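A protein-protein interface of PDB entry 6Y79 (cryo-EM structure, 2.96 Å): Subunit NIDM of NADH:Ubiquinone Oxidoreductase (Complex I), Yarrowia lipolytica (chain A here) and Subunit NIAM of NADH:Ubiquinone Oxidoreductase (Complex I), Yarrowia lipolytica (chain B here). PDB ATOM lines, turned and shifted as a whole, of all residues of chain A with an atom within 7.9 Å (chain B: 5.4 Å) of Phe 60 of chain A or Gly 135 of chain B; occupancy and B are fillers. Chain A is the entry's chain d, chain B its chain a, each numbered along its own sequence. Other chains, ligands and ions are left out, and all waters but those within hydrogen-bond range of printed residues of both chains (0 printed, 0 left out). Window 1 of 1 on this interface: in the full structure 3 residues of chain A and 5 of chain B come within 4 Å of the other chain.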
ATOM      1  N   CYS A  51     -10.167  -6.013  14.369  1.00  0.00           N
ATOM      2  CA  CYS A  51      -9.760  -5.366  15.622  1.00  0.00           C
ATOM      3  C   CYS A  51      -9.807  -6.328  16.798  1.00  0.00           C
ATOM      4  O   CYS A  51      -8.862  -6.405  17.588  1.00  0.00           O
ATOM      5  CB  CYS A  51     -10.649  -4.169  15.954  1.00  0.00           C
ATOM      6  SG  CYS A  51     -10.345  -3.651  17.682  1.00  0.00           S
ATOM      7  N   TYR A  52     -10.911  -7.062  16.922  1.00  0.00           N
ATOM      8  CA  TYR A  52     -11.088  -7.994  18.026  1.00  0.00           C
ATOM      9  C   TYR A  52     -10.073  -9.114  17.983  1.00  0.00           C
ATOM     10  O   TYR A  52      -9.522  -9.495  19.017  1.00  0.00           O
ATOM     11  CB  TYR A  52     -12.493  -8.571  18.007  1.00  0.00           C
ATOM     12  CG  TYR A  52     -12.759  -9.552  19.122  1.00  0.00           C
ATOM     13  CD1 TYR A  52     -12.999  -9.101  20.405  1.00  0.00           C
ATOM     14  CD2 TYR A  52     -12.771 -10.928  18.895  1.00  0.00           C
ATOM     15  CE1 TYR A  52     -13.247  -9.980  21.440  1.00  0.00           C
ATOM     16  CE2 TYR A  52     -13.014 -11.813  19.925  1.00  0.00           C
ATOM     17  CZ  TYR A  52     -13.252 -11.330  21.194  1.00  0.00           C
ATOM     18  OH  TYR A  52     -13.497 -12.190  22.236  1.00  0.00           O
ATOM     19  N   SER A  55      -6.712  -7.709  18.847  1.00  0.00           N
ATOM     20  CA  SER A  55      -6.540  -7.012  20.116  1.00  0.00           C
ATOM     21  C   SER A  55      -6.330  -7.986  21.259  1.00  0.00           C
ATOM     22  O   SER A  55      -5.468  -7.779  22.111  1.00  0.00           O
ATOM     23  CB  SER A  55      -7.735  -6.106  20.440  1.00  0.00           C
ATOM     24  OG  SER A  55      -7.545  -5.661  21.789  1.00  0.00           O
ATOM     25  N   GLY A  56      -7.147  -9.019  21.345  1.00  0.00           N
ATOM     26  CA  GLY A  56      -7.011  -9.970  22.426  1.00  0.00           C
ATOM     27  C   GLY A  56      -7.804  -9.544  23.639  1.00  0.00           C
ATOM     28  O   GLY A  56      -9.034  -9.598  23.633  1.00  0.00           O
ATOM     29  N   PRO A  57      -7.123  -9.143  24.710  1.00  0.00           N
ATOM     30  CA  PRO A  57      -7.849  -8.740  25.921  1.00  0.00           C
ATOM     31  C   PRO A  57      -8.309  -7.288  25.962  1.00  0.00           C
ATOM     32  O   PRO A  57      -9.315  -6.992  26.610  1.00  0.00           O
ATOM     33  CB  PRO A  57      -6.841  -9.035  27.038  1.00  0.00           C
ATOM     34  CG  PRO A  57      -5.530  -8.911  26.389  1.00  0.00           C
ATOM     35  CD  PRO A  57      -5.696  -9.383  24.979  1.00  0.00           C
ATOM     36  N   ASN A  58      -7.626  -6.367  25.282  1.00  0.00           N
ATOM     37  CA  ASN A  58      -7.942  -4.948  25.409  1.00  0.00           C
ATOM     38  C   ASN A  58      -8.867  -4.441  24.302  1.00  0.00           C
ATOM     39  O   ASN A  58      -8.918  -3.235  24.037  1.00  0.00           O
ATOM     40  CB  ASN A  58      -6.655  -4.121  25.470  1.00  0.00           C
ATOM     41  CG  ASN A  58      -5.674  -4.474  24.372  1.00  0.00           C
ATOM     42  OD1 ASN A  58      -5.959  -5.295  23.507  1.00  0.00           O
ATOM     43  ND2 ASN A  58      -4.500  -3.858  24.412  1.00  0.00           N
ATOM     44  N   HIS A  59      -9.641  -5.341  23.681  1.00  0.00           N
ATOM     45  CA  HIS A  59     -10.597  -4.980  22.637  1.00  0.00           C
ATOM     46  C   HIS A  59     -11.719  -4.100  23.148  1.00  0.00           C
ATOM     47  O   HIS A  59     -12.423  -3.476  22.345  1.00  0.00           O
ATOM     48  CB  HIS A  59     -11.192  -6.240  22.025  1.00  0.00           C
ATOM     49  CG  HIS A  59     -12.042  -7.030  22.970  1.00  0.00           C
ATOM     50  ND1 HIS A  59     -13.410  -6.885  23.054  1.00  0.00           N
ATOM     51  CD2 HIS A  59     -11.705  -7.958  23.891  1.00  0.00           C
ATOM     52  CE1 HIS A  59     -13.879  -7.700  23.980  1.00  0.00           C
ATOM     53  NE2 HIS A  59     -12.864  -8.364  24.501  1.00  0.00           N
ATOM     54  N   PHE A  60     -11.922  -4.076  24.461  1.00  0.00           N
ATOM     55  CA  PHE A  60     -12.847  -3.132  25.062  1.00  0.00           C
ATOM     56  C   PHE A  60     -12.429  -1.688  24.797  1.00  0.00           C
ATOM     57  O   PHE A  60     -13.275  -0.840  24.501  1.00  0.00           O
ATOM     58  CB  PHE A  60     -12.933  -3.415  26.553  1.00  0.00           C
ATOM     59  CG  PHE A  60     -13.454  -4.767  26.868  1.00  0.00           C
ATOM     60  CD1 PHE A  60     -14.800  -5.035  26.752  1.00  0.00           C
ATOM     61  CD2 PHE A  60     -12.598  -5.784  27.259  1.00  0.00           C
ATOM     62  CE1 PHE A  60     -15.290  -6.283  27.028  1.00  0.00           C
ATOM     63  CE2 PHE A  60     -13.087  -7.039  27.540  1.00  0.00           C
ATOM     64  CZ  PHE A  60     -14.437  -7.289  27.425  1.00  0.00           C
ATOM     65  N   GLU A  61     -11.131  -1.394  24.828  1.00  0.00           N
ATOM     66  CA  GLU A  61     -10.742   0.004  24.687  1.00  0.00           C
ATOM     67  C   GLU A  61     -10.052   0.338  23.378  1.00  0.00           C
ATOM     68  O   GLU A  61      -9.947   1.526  23.061  1.00  0.00           O
ATOM     69  CB  GLU A  61      -9.810   0.413  25.813  1.00  0.00           C
ATOM     70  CG  GLU A  61      -8.766  -0.592  25.886  1.00  0.00           C
ATOM     71  CD  GLU A  61      -7.846  -0.435  27.090  1.00  0.00           C
ATOM     72  OE1 GLU A  61      -7.155  -1.423  27.372  1.00  0.00           O
ATOM     73  OE2 GLU A  61      -7.834   0.658  27.660  1.00  0.00           O
ATOM     74  N   ASP A  62      -9.519  -0.645  22.643  1.00  0.00           N
ATOM     75  CA  ASP A  62      -8.988  -0.321  21.326  1.00  0.00           C
ATOM     76  C   ASP A  62     -10.121  -0.006  20.371  1.00  0.00           C
ATOM     77  O   ASP A  62     -10.082   1.017  19.695  1.00  0.00           O
ATOM     78  CB  ASP A  62      -8.114  -1.455  20.776  1.00  0.00           C
ATOM     79  CG  ASP A  62      -7.297  -1.039  19.523  1.00  0.00           C
ATOM     80  OD1 ASP A  62      -7.843  -0.540  18.497  1.00  0.00           O
ATOM     81  OD2 ASP A  62      -6.059  -1.177  19.571  1.00  0.00           O
ATOM     82  N   CYS A  63     -11.148  -0.841  20.313  1.00  0.00           N
ATOM     83  CA  CYS A  63     -12.243  -0.582  19.390  1.00  0.00           C
ATOM     84  C   CYS A  63     -13.569  -0.525  20.129  1.00  0.00           C
ATOM     85  O   CYS A  63     -14.516  -1.252  19.831  1.00  0.00           O
ATOM     86  CB  CYS A  63     -12.263  -1.562  18.224  1.00  0.00           C
ATOM     87  SG  CYS A  63     -12.171  -3.309  18.537  1.00  0.00           S
ATOM     88  N   LYS A  64     -13.627   0.327  21.149  1.00  0.00           N
ATOM     89  CA  LYS A  64     -14.929   0.806  21.591  1.00  0.00           C
ATOM     90  C   LYS A  64     -15.642   1.540  20.464  1.00  0.00           C
ATOM     91  O   LYS A  64     -16.820   1.281  20.207  1.00  0.00           O
ATOM     92  CB  LYS A  64     -14.808   1.712  22.816  1.00  0.00           C
ATOM     93  CG  LYS A  64     -16.161   2.012  23.431  1.00  0.00           C
ATOM     94  CD  LYS A  64     -16.044   2.768  24.727  1.00  0.00           C
ATOM     95  CE  LYS A  64     -17.409   3.204  25.221  1.00  0.00           C
ATOM     96  NZ  LYS A  64     -18.267   2.052  25.588  1.00  0.00           N
ATOM     97  N   ASN A  65     -14.933   2.412  19.740  1.00  0.00           N
ATOM     98  CA  ASN A  65     -15.600   3.240  18.736  1.00  0.00           C
ATOM     99  C   ASN A  65     -16.018   2.434  17.511  1.00  0.00           C
ATOM    100  O   ASN A  65     -17.060   2.720  16.917  1.00  0.00           O
ATOM    101  CB  ASN A  65     -14.710   4.411  18.319  1.00  0.00           C
ATOM    102  CG  ASN A  65     -14.569   5.457  19.405  1.00  0.00           C
ATOM    103  OD1 ASN A  65     -15.545   5.827  20.054  1.00  0.00           O
ATOM    104  ND2 ASN A  65     -13.352   5.947  19.599  1.00  0.00           N
ATOM    105  N   ALA A  67     -16.972  -0.739  17.655  1.00  0.00           N
ATOM    106  CA  ALA A  67     -18.126  -1.506  18.107  1.00  0.00           C
ATOM    107  C   ALA A  67     -19.368  -0.632  18.207  1.00  0.00           C
ATOM    108  O   ALA A  67     -20.461  -1.049  17.796  1.00  0.00           O
ATOM    109  CB  ALA A  67     -17.816  -2.159  19.451  1.00  0.00           C
ATOM    110  N   TRP B 131     -11.460   1.257  34.489  1.00  0.00           N
ATOM    111  CA  TRP B 131     -12.624   1.674  33.711  1.00  0.00           C
ATOM    112  C   TRP B 131     -12.237   1.982  32.267  1.00  0.00           C
ATOM    113  O   TRP B 131     -13.059   1.816  31.361  1.00  0.00           O
ATOM    114  CB  TRP B 131     -13.310   2.879  34.394  1.00  0.00           C
ATOM    115  CG  TRP B 131     -12.375   4.044  34.509  1.00  0.00           C
ATOM    116  CD1 TRP B 131     -11.569   4.347  35.540  1.00  0.00           C
ATOM    117  CD2 TRP B 131     -12.108   5.020  33.494  1.00  0.00           C
ATOM    118  NE1 TRP B 131     -10.812   5.461  35.252  1.00  0.00           N
ATOM    119  CE2 TRP B 131     -11.114   5.886  33.987  1.00  0.00           C
ATOM    120  CE3 TRP B 131     -12.605   5.230  32.197  1.00  0.00           C
ATOM    121  CZ2 TRP B 131     -10.628   6.946  33.243  1.00  0.00           C
ATOM    122  CZ3 TRP B 131     -12.087   6.277  31.455  1.00  0.00           C
ATOM    123  CH2 TRP B 131     -11.138   7.127  32.005  1.00  0.00           C
ATOM    124  N   LYS B 132     -11.015   2.483  32.042  1.00  0.00           N
ATOM    125  CA  LYS B 132     -10.569   2.742  30.680  1.00  0.00           C
ATOM    126  C   LYS B 132     -10.271   1.439  29.982  1.00  0.00           C
ATOM    127  O   LYS B 132     -10.470   1.316  28.774  1.00  0.00           O
ATOM    128  CB  LYS B 132      -9.339   3.654  30.680  1.00  0.00           C
ATOM    129  CG  LYS B 132      -8.819   4.062  29.294  1.00  0.00           C
ATOM    130  CD  LYS B 132      -7.635   5.013  29.409  1.00  0.00           C
ATOM    131  CE  LYS B 132      -7.104   5.432  28.047  1.00  0.00           C
ATOM    132  NZ  LYS B 132      -6.806   4.260  27.187  1.00  0.00           N
ATOM    133  N   GLU B 133      -9.821   0.453  30.747  1.00  0.00           N
ATOM    134  CA  GLU B 133      -9.561  -0.875  30.228  1.00  0.00           C
ATOM    135  C   GLU B 133     -10.848  -1.615  29.904  1.00  0.00           C
ATOM    136  O   GLU B 133     -10.865  -2.440  28.985  1.00  0.00           O
ATOM    137  CB  GLU B 133      -8.728  -1.631  31.257  1.00  0.00           C
ATOM    138  CG  GLU B 133      -7.398  -0.939  31.503  1.00  0.00           C
ATOM    139  CD  GLU B 133      -6.386  -1.201  30.404  1.00  0.00           C
ATOM    140  OE1 GLU B 133      -6.288  -2.360  29.959  1.00  0.00           O
ATOM    141  OE2 GLU B 133      -5.740  -0.232  29.957  1.00  0.00           O
ATOM    142  N   SER B 134     -11.928  -1.327  30.627  1.00  0.00           N
ATOM    143  CA  SER B 134     -13.220  -1.974  30.403  1.00  0.00           C
ATOM    144  C   SER B 134     -14.097  -1.136  29.474  1.00  0.00           C
ATOM    145  O   SER B 134     -15.261  -0.870  29.750  1.00  0.00           O
ATOM    146  CB  SER B 134     -13.922  -2.212  31.731  1.00  0.00           C
ATOM    147  OG  SER B 134     -13.168  -3.066  32.565  1.00  0.00           O
ATOM    148  N   GLY B 135     -13.528  -0.739  28.342  1.00  0.00           N
ATOM    149  CA  GLY B 135     -14.207   0.156  27.435  1.00  0.00           C
ATOM    150  C   GLY B 135     -14.207   1.534  28.041  1.00  0.00           C
ATOM    151  O   GLY B 135     -13.140   2.075  28.328  1.00  0.00           O
ATOM    152  N   GLY B 136     -15.385   2.104  28.251  1.00  0.00           N
ATOM    153  CA  GLY B 136     -15.521   3.256  29.119  1.00  0.00           C
ATOM    154  C   GLY B 136     -14.975   4.581  28.637  1.00  0.00           C
ATOM    155  O   GLY B 136     -14.112   4.658  27.772  1.00  0.00           O
ATOM    156  N   THR B 137     -15.541   5.649  29.170  1.00  0.00           N
ATOM    157  CA  THR B 137     -14.912   6.956  29.288  1.00  0.00           C
ATOM    158  C   THR B 137     -15.449   7.559  30.589  1.00  0.00           C
ATOM    159  O   THR B 137     -16.178   6.905  31.339  1.00  0.00           O
ATOM    160  CB  THR B 137     -15.169   7.847  28.044  1.00  0.00           C
ATOM    161  OG1 THR B 137     -14.591   9.148  28.221  1.00  0.00           O
ATOM    162  CG2 THR B 137     -16.634   7.968  27.741  1.00  0.00           C
ATOM    163  N   PHE B 144     -19.326   1.070  33.362  1.00  0.00           N
ATOM    164  CA  PHE B 144     -18.222   0.162  33.098  1.00  0.00           C
ATOM    165  C   PHE B 144     -17.130   0.464  34.125  1.00  0.00           C
ATOM    166  O   PHE B 144     -16.172   1.185  33.845  1.00  0.00           O
ATOM    167  CB  PHE B 144     -17.699   0.323  31.665  1.00  0.00           C
ATOM    168  CG  PHE B 144     -18.770   0.310  30.601  1.00  0.00           C
ATOM    169  CD1 PHE B 144     -19.382   1.486  30.192  1.00  0.00           C
ATOM    170  CD2 PHE B 144     -19.136  -0.875  29.984  1.00  0.00           C
ATOM    171  CE1 PHE B 144     -20.358   1.472  29.214  1.00  0.00           C
ATOM    172  CE2 PHE B 144     -20.109  -0.891  28.999  1.00  0.00           C
ATOM    173  CZ  PHE B 144     -20.719   0.284  28.615  1.00  0.00           C
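Of chain B, only Glu 133, Ser 134 and Gly 135 come within 4 Å of Phe 60 of chain A.
Of the printed residues of chain B, Glu 61 of chain A touches Lys 132 and Glu 133.
Of the printed residues of chain B, Lys 64 of chain A touches Gly 135 and Gly 136.
Printed residues of chain A within 4 Å of Lys 132 of chain B: Glu 61 (2.9 Å).
Of the printed residues of chain A, Glu 133 of chain B touches Phe 60 (3.3 Å) and Glu 61 (2.9 Å).
Of the printed residues of chain A, Ser 134 of chain B touches Phe 60 (3.9 Å).
Of the printed residues of chain A, Gly 135 of chain B touches Phe 60 (3.2 Å) and Lys 64 (3.98 Å).
The nearest printed residue of chain A that does not touch Glu 133 of chain B is Asn 58 of chain A (4.8 Å).
Of the 14 printed residues of chain A, 3 touch a printed residue of chain B.
Of the 8 printed residues of chain B, 5 touch a printed residue of chain A.
Printed residues of chain B that touch a printed residue of chain A: Lys 132, Glu 133, Ser 134, Gly 135 and Gly 136.
The side-chain sulfur (SG) of Cys 63 of chain A is disulfide-bonded to the side-chain sulfur (SG) of Cys 51 of chain A.
Among the printed residues, merely in contact across the chains: Phe 60 of chain A with Glu 133 of chain B, Phe 60 of chain A with Ser 134 of chain B, Phe 60 of chain A with Gly 135 of chain B, Lys 64 of chain A with Gly 135 of chain B and Lys 64 of chain A with Gly 136 of chain B.
The side-chain carboxylate (OE1) of Glu 133 of chain B sits close to the side-chain carboxylate (OE1) of Glu 61 of chain A (2.9 Å).
NZ of Lys 132 of chain B is in salt-bridge range of OE2 of Glu 61 of chain A, 3.8 Å away.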
